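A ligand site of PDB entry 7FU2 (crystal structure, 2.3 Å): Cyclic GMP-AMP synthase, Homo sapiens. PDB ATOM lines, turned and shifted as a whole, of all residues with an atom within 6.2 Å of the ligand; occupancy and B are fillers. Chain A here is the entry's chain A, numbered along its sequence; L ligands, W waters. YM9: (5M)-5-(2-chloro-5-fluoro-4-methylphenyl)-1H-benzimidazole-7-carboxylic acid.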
ATOM      1  N   LYS A  59     -31.685 -21.886  21.411  1.00  0.00           N
ATOM      2  CA  LYS A  59     -31.271 -20.628  20.785  1.00  0.00           C
ATOM      3  C   LYS A  59     -30.957 -20.852  19.285  1.00  0.00           C
ATOM      4  O   LYS A  59     -30.888 -22.001  18.847  1.00  0.00           O
ATOM      5  CB  LYS A  59     -30.039 -20.099  21.525  1.00  0.00           C
ATOM      6  CG  LYS A  59     -29.990 -18.582  21.690  1.00  0.00           C
ATOM      7  CD  LYS A  59     -28.867 -18.172  22.637  1.00  0.00           C
ATOM      8  CE  LYS A  59     -27.510 -18.092  21.964  1.00  0.00           C
ATOM      9  NZ  LYS A  59     -26.403 -18.077  22.961  1.00  0.00           N
ATOM     10  N   ASP A  67     -28.084 -23.318  19.488  1.00  0.00           N
ATOM     11  CA  ASP A  67     -27.212 -23.199  20.658  1.00  0.00           C
ATOM     12  C   ASP A  67     -27.872 -23.675  21.938  1.00  0.00           C
ATOM     13  O   ASP A  67     -28.863 -23.100  22.383  1.00  0.00           O
ATOM     14  CB  ASP A  67     -26.689 -21.755  20.804  1.00  0.00           C
ATOM     15  CG  ASP A  67     -25.215 -21.597  20.490  1.00  0.00           C
ATOM     16  OD1 ASP A  67     -24.834 -21.780  19.305  1.00  0.00           O
ATOM     17  OD2 ASP A  67     -24.445 -21.299  21.424  1.00  0.00           O
ATOM     18  N   LEU A 178     -22.437  -3.779  30.881  1.00  0.00           N
ATOM     19  CA  LEU A 178     -23.910  -3.681  30.890  1.00  0.00           C
ATOM     20  C   LEU A 178     -24.385  -2.215  31.095  1.00  0.00           C
ATOM     21  O   LEU A 178     -25.183  -1.942  31.985  1.00  0.00           O
ATOM     22  CB  LEU A 178     -24.505  -4.648  31.950  1.00  0.00           C
ATOM     23  CG  LEU A 178     -26.014  -5.000  31.878  1.00  0.00           C
ATOM     24  CD1 LEU A 178     -26.387  -5.727  30.578  1.00  0.00           C
ATOM     25  CD2 LEU A 178     -26.424  -5.810  33.093  1.00  0.00           C
ATOM     26  N   ILE A 180     -26.565   0.026  30.619  1.00  0.00           N
ATOM     27  CA  ILE A 180     -27.967   0.171  30.266  1.00  0.00           C
ATOM     28  C   ILE A 180     -28.681   1.239  31.108  1.00  0.00           C
ATOM     29  O   ILE A 180     -29.844   1.525  30.820  1.00  0.00           O
ATOM     30  CB  ILE A 180     -28.690  -1.219  30.316  1.00  0.00           C
ATOM     31  CG1 ILE A 180     -28.640  -1.855  31.740  1.00  0.00           C
ATOM     32  CG2 ILE A 180     -28.133  -2.169  29.234  1.00  0.00           C
ATOM     33  CD1 ILE A 180     -29.637  -2.984  31.950  1.00  0.00           C
ATOM     34  N   TRP A 183     -30.788   3.759  29.407  1.00  0.00           N
ATOM     35  CA  TRP A 183     -31.707   3.115  28.463  1.00  0.00           C
ATOM     36  C   TRP A 183     -32.788   2.310  29.226  1.00  0.00           C
ATOM     37  O   TRP A 183     -33.954   2.722  29.270  1.00  0.00           O
ATOM     38  CB  TRP A 183     -30.886   2.271  27.442  1.00  0.00           C
ATOM     39  CG  TRP A 183     -31.621   1.225  26.654  1.00  0.00           C
ATOM     40  CD1 TRP A 183     -32.895   1.297  26.183  1.00  0.00           C
ATOM     41  CD2 TRP A 183     -31.091  -0.025  26.197  1.00  0.00           C
ATOM     42  NE1 TRP A 183     -33.214   0.141  25.498  1.00  0.00           N
ATOM     43  CE2 TRP A 183     -32.134  -0.696  25.511  1.00  0.00           C
ATOM     44  CE3 TRP A 183     -29.854  -0.683  26.349  1.00  0.00           C
ATOM     45  CZ2 TRP A 183     -31.977  -1.976  24.967  1.00  0.00           C
ATOM     46  CZ3 TRP A 183     -29.691  -1.954  25.817  1.00  0.00           C
ATOM     47  CH2 TRP A 183     -30.749  -2.595  25.143  1.00  0.00           C
ATOM     48  N   VAL A 200     -17.731 -20.823  30.951  1.00  0.00           N
ATOM     49  CA  VAL A 200     -17.631 -21.760  29.830  1.00  0.00           C
ATOM     50  C   VAL A 200     -16.156 -22.100  29.482  1.00  0.00           C
ATOM     51  O   VAL A 200     -15.321 -21.199  29.528  1.00  0.00           O
ATOM     52  CB  VAL A 200     -18.433 -21.294  28.576  1.00  0.00           C
ATOM     53  CG1 VAL A 200     -19.931 -21.344  28.839  1.00  0.00           C
ATOM     54  CG2 VAL A 200     -18.002 -19.911  28.113  1.00  0.00           C
ATOM     55  N   ARG A 216     -14.179 -18.870  30.485  1.00  0.00           N
ATOM     56  CA  ARG A 216     -14.642 -17.551  30.058  1.00  0.00           C
ATOM     57  C   ARG A 216     -16.000 -17.222  30.689  1.00  0.00           C
ATOM     58  O   ARG A 216     -16.843 -18.106  30.794  1.00  0.00           O
ATOM     59  CB  ARG A 216     -14.732 -17.508  28.521  1.00  0.00           C
ATOM     60  CG  ARG A 216     -15.077 -16.135  27.930  1.00  0.00           C
ATOM     61  CD  ARG A 216     -15.470 -16.167  26.460  1.00  0.00           C
ATOM     62  NE  ARG A 216     -16.638 -17.025  26.190  1.00  0.00           N
ATOM     63  CZ  ARG A 216     -17.908 -16.623  26.225  1.00  0.00           C
ATOM     64  NH1 ARG A 216     -18.219 -15.366  26.536  1.00  0.00           N
ATOM     65  NH2 ARG A 216     -18.889 -17.473  25.945  1.00  0.00           N
ATOM     66  N   LEU A 217     -16.214 -15.939  31.087  1.00  0.00           N
ATOM     67  CA  LEU A 217     -17.475 -15.449  31.646  1.00  0.00           C
ATOM     68  C   LEU A 217     -18.502 -15.351  30.547  1.00  0.00           C
ATOM     69  O   LEU A 217     -18.238 -14.739  29.503  1.00  0.00           O
ATOM     70  CB  LEU A 217     -17.322 -14.056  32.269  1.00  0.00           C
ATOM     71  CG  LEU A 217     -16.418 -13.877  33.483  1.00  0.00           C
ATOM     72  CD1 LEU A 217     -16.336 -12.404  33.844  1.00  0.00           C
ATOM     73  CD2 LEU A 217     -16.887 -14.723  34.676  1.00  0.00           C
ATOM     74  N   SER A 218     -19.679 -15.960  30.775  1.00  0.00           N
ATOM     75  CA  SER A 218     -20.781 -15.965  29.826  1.00  0.00           C
ATOM     76  C   SER A 218     -22.024 -15.353  30.437  1.00  0.00           C
ATOM     77  O   SER A 218     -22.353 -15.610  31.606  1.00  0.00           O
ATOM     78  CB  SER A 218     -21.081 -17.373  29.340  1.00  0.00           C
ATOM     79  OG  SER A 218     -22.075 -17.284  28.328  1.00  0.00           O
ATOM     80  N   PHE A 219     -22.695 -14.525  29.635  1.00  0.00           N
ATOM     81  CA  PHE A 219     -23.898 -13.802  30.021  1.00  0.00           C
ATOM     82  C   PHE A 219     -24.966 -13.887  28.947  1.00  0.00           C
ATOM     83  O   PHE A 219     -25.775 -12.974  28.825  1.00  0.00           O
ATOM     84  CB  PHE A 219     -23.528 -12.340  30.283  1.00  0.00           C
ATOM     85  CG  PHE A 219     -22.529 -12.120  31.393  1.00  0.00           C
ATOM     86  CD1 PHE A 219     -22.945 -12.045  32.713  1.00  0.00           C
ATOM     87  CD2 PHE A 219     -21.174 -11.961  31.106  1.00  0.00           C
ATOM     88  CE1 PHE A 219     -22.019 -11.831  33.739  1.00  0.00           C
ATOM     89  CE2 PHE A 219     -20.256 -11.751  32.129  1.00  0.00           C
ATOM     90  CZ  PHE A 219     -20.685 -11.695  33.442  1.00  0.00           C
ATOM     91  N   SER A 220     -24.987 -14.998  28.173  1.00  0.00           N
ATOM     92  CA  SER A 220     -25.925 -15.233  27.064  1.00  0.00           C
ATOM     93  C   SER A 220     -27.359 -15.355  27.530  1.00  0.00           C
ATOM     94  O   SER A 220     -28.280 -15.063  26.765  1.00  0.00           O
ATOM     95  CB  SER A 220     -25.523 -16.473  26.254  1.00  0.00           C
ATOM     96  OG  SER A 220     -25.342 -17.590  27.116  1.00  0.00           O
ATOM     97  N   HIS A 221     -27.549 -15.785  28.772  1.00  0.00           N
ATOM     98  CA  HIS A 221     -28.846 -15.954  29.426  1.00  0.00           C
ATOM     99  C   HIS A 221     -29.531 -14.602  29.692  1.00  0.00           C
ATOM    100  O   HIS A 221     -30.748 -14.552  29.823  1.00  0.00           O
ATOM    101  CB  HIS A 221     -28.660 -16.754  30.739  1.00  0.00           C
ATOM    102  CG  HIS A 221     -27.867 -16.034  31.788  1.00  0.00           C
ATOM    103  ND1 HIS A 221     -26.514 -15.790  31.628  1.00  0.00           N
ATOM    104  CD2 HIS A 221     -28.257 -15.554  32.982  1.00  0.00           C
ATOM    105  CE1 HIS A 221     -26.134 -15.145  32.713  1.00  0.00           C
ATOM    106  NE2 HIS A 221     -27.157 -14.990  33.570  1.00  0.00           N
ATOM    107  N   ILE A 222     -28.754 -13.519  29.752  1.00  0.00           N
ATOM    108  CA  ILE A 222     -29.275 -12.171  29.991  1.00  0.00           C
ATOM    109  C   ILE A 222     -29.958 -11.610  28.743  1.00  0.00           C
ATOM    110  O   ILE A 222     -30.875 -10.795  28.878  1.00  0.00           O
ATOM    111  CB  ILE A 222     -28.160 -11.222  30.586  1.00  0.00           C
ATOM    112  CG1 ILE A 222     -27.519 -11.802  31.888  1.00  0.00           C
ATOM    113  CG2 ILE A 222     -28.624  -9.762  30.800  1.00  0.00           C
ATOM    114  CD1 ILE A 222     -28.434 -11.925  33.119  1.00  0.00           C
ATOM    115  N   GLU A 223     -29.554 -12.059  27.537  1.00  0.00           N
ATOM    116  CA  GLU A 223     -30.102 -11.578  26.266  1.00  0.00           C
ATOM    117  C   GLU A 223     -31.644 -11.659  26.169  1.00  0.00           C
ATOM    118  O   GLU A 223     -32.268 -10.693  25.741  1.00  0.00           O
ATOM    119  CB  GLU A 223     -29.433 -12.262  25.084  1.00  0.00           C
ATOM    120  CG  GLU A 223     -29.675 -11.547  23.767  1.00  0.00           C
ATOM    121  CD  GLU A 223     -29.331 -12.294  22.493  1.00  0.00           C
ATOM    122  OE1 GLU A 223     -28.825 -13.441  22.573  1.00  0.00           O
ATOM    123  OE2 GLU A 223     -29.587 -11.733  21.402  1.00  0.00           O
ATOM    124  N   LYS A 224     -32.246 -12.813  26.559  1.00  0.00           N
ATOM    125  CA  LYS A 224     -33.708 -13.020  26.527  1.00  0.00           C
ATOM    126  C   LYS A 224     -34.441 -12.018  27.474  1.00  0.00           C
ATOM    127  O   LYS A 224     -35.582 -11.635  27.217  1.00  0.00           O
ATOM    128  CB  LYS A 224     -34.063 -14.483  26.873  1.00  0.00           C
ATOM    129  CG  LYS A 224     -33.733 -14.897  28.310  1.00  0.00           C
ATOM    130  CD  LYS A 224     -33.922 -16.354  28.573  1.00  0.00           C
ATOM    131  CE  LYS A 224     -33.960 -16.611  30.056  1.00  0.00           C
ATOM    132  NZ  LYS A 224     -35.355 -16.662  30.564  1.00  0.00           N
ATOM    133  N   ILE A 226     -33.507  -8.832  28.181  1.00  0.00           N
ATOM    134  CA  ILE A 226     -33.454  -7.520  27.553  1.00  0.00           C
ATOM    135  C   ILE A 226     -34.226  -7.456  26.237  1.00  0.00           C
ATOM    136  O   ILE A 226     -34.933  -6.469  26.022  1.00  0.00           O
ATOM    137  CB  ILE A 226     -31.979  -7.063  27.430  1.00  0.00           C
ATOM    138  CG1 ILE A 226     -31.422  -6.729  28.843  1.00  0.00           C
ATOM    139  CG2 ILE A 226     -31.802  -5.874  26.468  1.00  0.00           C
ATOM    140  CD1 ILE A 226     -29.941  -6.570  28.979  1.00  0.00           C
ATOM    141  N   SER A 275     -22.994 -14.521  15.106  1.00  0.00           N
ATOM    142  CA  SER A 275     -24.152 -13.728  15.551  1.00  0.00           C
ATOM    143  C   SER A 275     -23.829 -12.930  16.821  1.00  0.00           C
ATOM    144  O   SER A 275     -24.362 -11.832  16.999  1.00  0.00           O
ATOM    145  CB  SER A 275     -25.351 -14.638  15.806  1.00  0.00           C
ATOM    146  OG  SER A 275     -25.129 -15.508  16.899  1.00  0.00           O
ATOM    147  N   TYR A 276     -22.907 -13.466  17.656  1.00  0.00           N
ATOM    148  CA  TYR A 276     -22.420 -12.870  18.915  1.00  0.00           C
ATOM    149  C   TYR A 276     -21.813 -11.484  18.706  1.00  0.00           C
ATOM    150  O   TYR A 276     -22.057 -10.588  19.511  1.00  0.00           O
ATOM    151  CB  TYR A 276     -21.429 -13.827  19.616  1.00  0.00           C
ATOM    152  CG  TYR A 276     -20.771 -13.277  20.876  1.00  0.00           C
ATOM    153  CD1 TYR A 276     -21.546 -12.716  21.898  1.00  0.00           C
ATOM    154  CD2 TYR A 276     -19.409 -13.396  21.077  1.00  0.00           C
ATOM    155  CE1 TYR A 276     -20.951 -12.203  23.046  1.00  0.00           C
ATOM    156  CE2 TYR A 276     -18.815 -12.936  22.255  1.00  0.00           C
ATOM    157  CZ  TYR A 276     -19.581 -12.332  23.232  1.00  0.00           C
ATOM    158  OH  TYR A 276     -18.999 -11.838  24.371  1.00  0.00           O
ATOM    159  N   LYS A 279     -24.695  -9.113  17.624  1.00  0.00           N
ATOM    160  CA  LYS A 279     -25.493  -8.825  18.824  1.00  0.00           C
ATOM    161  C   LYS A 279     -24.803  -7.762  19.667  1.00  0.00           C
ATOM    162  O   LYS A 279     -25.417  -6.756  19.998  1.00  0.00           O
ATOM    163  CB  LYS A 279     -25.689 -10.080  19.676  1.00  0.00           C
ATOM    164  CG  LYS A 279     -26.758 -11.047  19.204  1.00  0.00           C
ATOM    165  CD  LYS A 279     -26.659 -12.309  20.034  1.00  0.00           C
ATOM    166  CE  LYS A 279     -27.448 -13.455  19.470  1.00  0.00           C
ATOM    167  NZ  LYS A 279     -27.384 -14.641  20.364  1.00  0.00           N
ATOM    168  N   THR A 280     -23.501  -7.995  20.019  1.00  0.00           N
ATOM    169  CA  THR A 280     -22.678  -7.077  20.814  1.00  0.00           C
ATOM    170  C   THR A 280     -22.733  -5.676  20.217  1.00  0.00           C
ATOM    171  O   THR A 280     -23.107  -4.753  20.912  1.00  0.00           O
ATOM    172  CB  THR A 280     -21.241  -7.624  20.940  1.00  0.00           C
ATOM    173  OG1 THR A 280     -21.284  -8.900  21.565  1.00  0.00           O
ATOM    174  CG2 THR A 280     -20.351  -6.722  21.752  1.00  0.00           C
ATOM    175  N   PHE A 283     -26.360  -4.051  20.469  1.00  0.00           N
ATOM    176  CA  PHE A 283     -26.626  -3.597  21.831  1.00  0.00           C
ATOM    177  C   PHE A 283     -25.807  -2.364  22.194  1.00  0.00           C
ATOM    178  O   PHE A 283     -26.335  -1.503  22.885  1.00  0.00           O
ATOM    179  CB  PHE A 283     -26.490  -4.743  22.841  1.00  0.00           C
ATOM    180  CG  PHE A 283     -27.647  -5.729  22.794  1.00  0.00           C
ATOM    181  CD1 PHE A 283     -28.924  -5.351  23.208  1.00  0.00           C
ATOM    182  CD2 PHE A 283     -27.462  -7.026  22.326  1.00  0.00           C
ATOM    183  CE1 PHE A 283     -29.975  -6.262  23.159  1.00  0.00           C
ATOM    184  CE2 PHE A 283     -28.526  -7.936  22.282  1.00  0.00           C
ATOM    185  CZ  PHE A 283     -29.776  -7.548  22.704  1.00  0.00           C
ATOM    186  N   ASN A 322     -16.604  -6.320  24.581  1.00  0.00           N
ATOM    187  CA  ASN A 322     -17.564  -7.273  25.152  1.00  0.00           C
ATOM    188  C   ASN A 322     -18.567  -6.431  25.940  1.00  0.00           C
ATOM    189  O   ASN A 322     -18.165  -5.541  26.699  1.00  0.00           O
ATOM    190  CB  ASN A 322     -16.837  -8.260  26.066  1.00  0.00           C
ATOM    191  CG  ASN A 322     -17.702  -9.327  26.715  1.00  0.00           C
ATOM    192  OD1 ASN A 322     -18.803  -9.089  27.226  1.00  0.00           O
ATOM    193  ND2 ASN A 322     -17.184 -10.534  26.721  1.00  0.00           N
ATOM    194  N   TYR A 323     -19.880  -6.654  25.726  1.00  0.00           N
ATOM    195  CA  TYR A 323     -20.953  -5.890  26.360  1.00  0.00           C
ATOM    196  C   TYR A 323     -20.959  -5.910  27.897  1.00  0.00           C
ATOM    197  O   TYR A 323     -21.460  -4.971  28.518  1.00  0.00           O
ATOM    198  CB  TYR A 323     -22.323  -6.327  25.824  1.00  0.00           C
ATOM    199  CG  TYR A 323     -23.364  -5.241  25.937  1.00  0.00           C
ATOM    200  CD1 TYR A 323     -23.373  -4.158  25.057  1.00  0.00           C
ATOM    201  CD2 TYR A 323     -24.323  -5.273  26.952  1.00  0.00           C
ATOM    202  CE1 TYR A 323     -24.293  -3.129  25.203  1.00  0.00           C
ATOM    203  CE2 TYR A 323     -25.261  -4.250  27.093  1.00  0.00           C
ATOM    204  CZ  TYR A 323     -25.242  -3.178  26.208  1.00  0.00           C
ATOM    205  OH  TYR A 323     -26.178  -2.186  26.304  1.00  0.00           O
ATOM    206  N   PHE A 324     -20.378  -6.942  28.508  1.00  0.00           N
ATOM    207  CA  PHE A 324     -20.348  -7.120  29.967  1.00  0.00           C
ATOM    208  C   PHE A 324     -18.991  -6.844  30.555  1.00  0.00           C
ATOM    209  O   PHE A 324     -18.903  -6.586  31.745  1.00  0.00           O
ATOM    210  CB  PHE A 324     -20.818  -8.533  30.339  1.00  0.00           C
ATOM    211  CG  PHE A 324     -22.263  -8.782  30.008  1.00  0.00           C
ATOM    212  CD1 PHE A 324     -22.649  -9.114  28.721  1.00  0.00           C
ATOM    213  CD2 PHE A 324     -23.248  -8.648  30.987  1.00  0.00           C
ATOM    214  CE1 PHE A 324     -23.990  -9.291  28.401  1.00  0.00           C
ATOM    215  CE2 PHE A 324     -24.591  -8.857  30.673  1.00  0.00           C
ATOM    216  CZ  PHE A 324     -24.952  -9.163  29.383  1.00  0.00           C
HETATM  217  C10 YM9 L   1     -23.556 -12.504  25.906  1.00  0.00           C
HETATM  218  C11 YM9 L   1     -21.662 -14.048  26.507  1.00  0.00           C
HETATM  219  O12 YM9 L   1     -21.388 -13.296  27.486  1.00  0.00           O
HETATM  220  C17 YM9 L   1     -23.213 -14.448  24.518  1.00  0.00           C
HETATM  221  C18 YM9 L   1     -24.298 -14.070  23.719  1.00  0.00           C
HETATM  222  C20 YM9 L   1     -23.492 -15.918  22.945  1.00  0.00           C
HETATM  223  C1  YM9 L   1     -25.798  -8.477  24.918  1.00  0.00           C
HETATM  224  C14 YM9 L   1     -27.441  -7.122  26.267  1.00  0.00           C
HETATM  225  C2  YM9 L   1     -26.716  -8.405  25.968  1.00  0.00           C
HETATM  226  C3  YM9 L   1     -26.920  -9.564  26.694  1.00  0.00           C
HETATM  227  C4  YM9 L   1     -26.280 -10.756  26.424  1.00  0.00           C
HETATM  228  C5  YM9 L   1     -25.352 -10.832  25.382  1.00  0.00           C
HETATM  229  C6  YM9 L   1     -25.151  -9.670  24.627  1.00  0.00           C
HETATM  230  C7  YM9 L   1     -24.649 -12.116  25.123  1.00  0.00           C
HETATM  231  C8  YM9 L   1     -25.007 -12.895  24.015  1.00  0.00           C
HETATM  232  C9  YM9 L   1     -22.843 -13.691  25.645  1.00  0.00           C
HETATM  233  F15 YM9 L   1     -27.769  -9.524  27.736  1.00  0.00           F
HETATM  234  N19 YM9 L   1     -24.423 -15.007  22.685  1.00  0.00           N
HETATM  235  N21 YM9 L   1     -22.742 -15.631  24.028  1.00  0.00           N
HETATM  236  O13 YM9 L   1     -20.992 -15.064  26.185  1.00  0.00           O
HETATM  237 CL16 YM9 L   1     -24.008  -9.667  23.330  1.00  0.00          CL
HETATM  238  O   HOH W   1     -20.608 -10.949  26.373  1.00  0.00           O
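O of Val 200 lies within hydrogen-bond range of N of Arg 216, at 2.8 Å.
NZ of Lys 279 lies within salt-bridge range of OE1 of Glu 223.
The side-chain hydroxyl (OG) of Ser 218 sits at hydrogen-bond distance from the side-chain hydroxyl (OG) of Ser 220 (3.5 Å).
The backbone NH of Phe 324 sits at hydrogen-bond distance from the side-chain amide oxygen of Asn 322, 3.0 Å away.
O of Phe 283 sits at hydrogen-bond distance from OH of Tyr 323.
The side-chain hydroxyl (OH) of Tyr 276 lies within hydrogen-bond range of the side-chain amide nitrogen (ND2) of Asn 322, at 3.2 Å.
The backbone carbonyl oxygen (O) of Lys 59 is in hydrogen-bond range of the backbone NH (N) of Asp 67.
The backbone carbonyl oxygen (O) of Tyr 323 lies within hydrogen-bond range of the backbone NH (N) of Leu 178 (2.8 Å).
The backbone NH (N) of Glu 223 sits close to a fluorine (F15) of the ligand (3.1 Å).
NZ of Lys 59 touches C20 of the ligand, 3.6 Å away.
Ser 220 touches the ligand (CB to C17, 3.5 Å).
Ile 222 touches the ligand (C to F15, 3.2 Å).
CD1 of Ile 226 touches C14 of the ligand (3.7 Å).
Tyr 276 touches the ligand (CE1 to C17, 3.5 Å).
NZ of Lys 279 touches N19 of the ligand, 3.8 Å away.
Thr 280 touches the ligand.
Phe 283 touches the ligand (CD2 to C1, 3.4 Å).
Tyr 323 touches the ligand (CD2 to C14, 3.7 Å).
Phe 324 touches the ligand (CZ to F15, 3.3 Å).
Hydrophobic or aromatic side chains within 4 Å of the ligand: Phe 219, Ile 222, Ile 226, Tyr 276, Phe 283, Tyr 323 and Phe 324.
Within 4 Å of the ligand: Lys 59, Arg 216, Ser 218, Phe 219, Ser 220, Ile 222, Glu 223, Ile 226, Tyr 276, Lys 279, Thr 280, Phe 283, Tyr 323 and Phe 324.
The nearest printed residue that does not touch the ligand is Leu 217 (4.01 Å).
An oxygen (O12) of the ligand sits at hydrogen-bond distance from the backbone NH (N) of Phe 219 (2.8 Å).
O13 of the ligand lies within salt-bridge range of NH1 of Arg 216 (2.8 Å).
The side-chain hydroxyl (OG) of Ser 218 lies within hydrogen-bond range of an oxygen (O13) of the ligand, 3.3 Å away.
Water W1 lies within hydrogen-bond range of O12 of the ligand, OH of Tyr 276 and OD1 of Asn 322.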
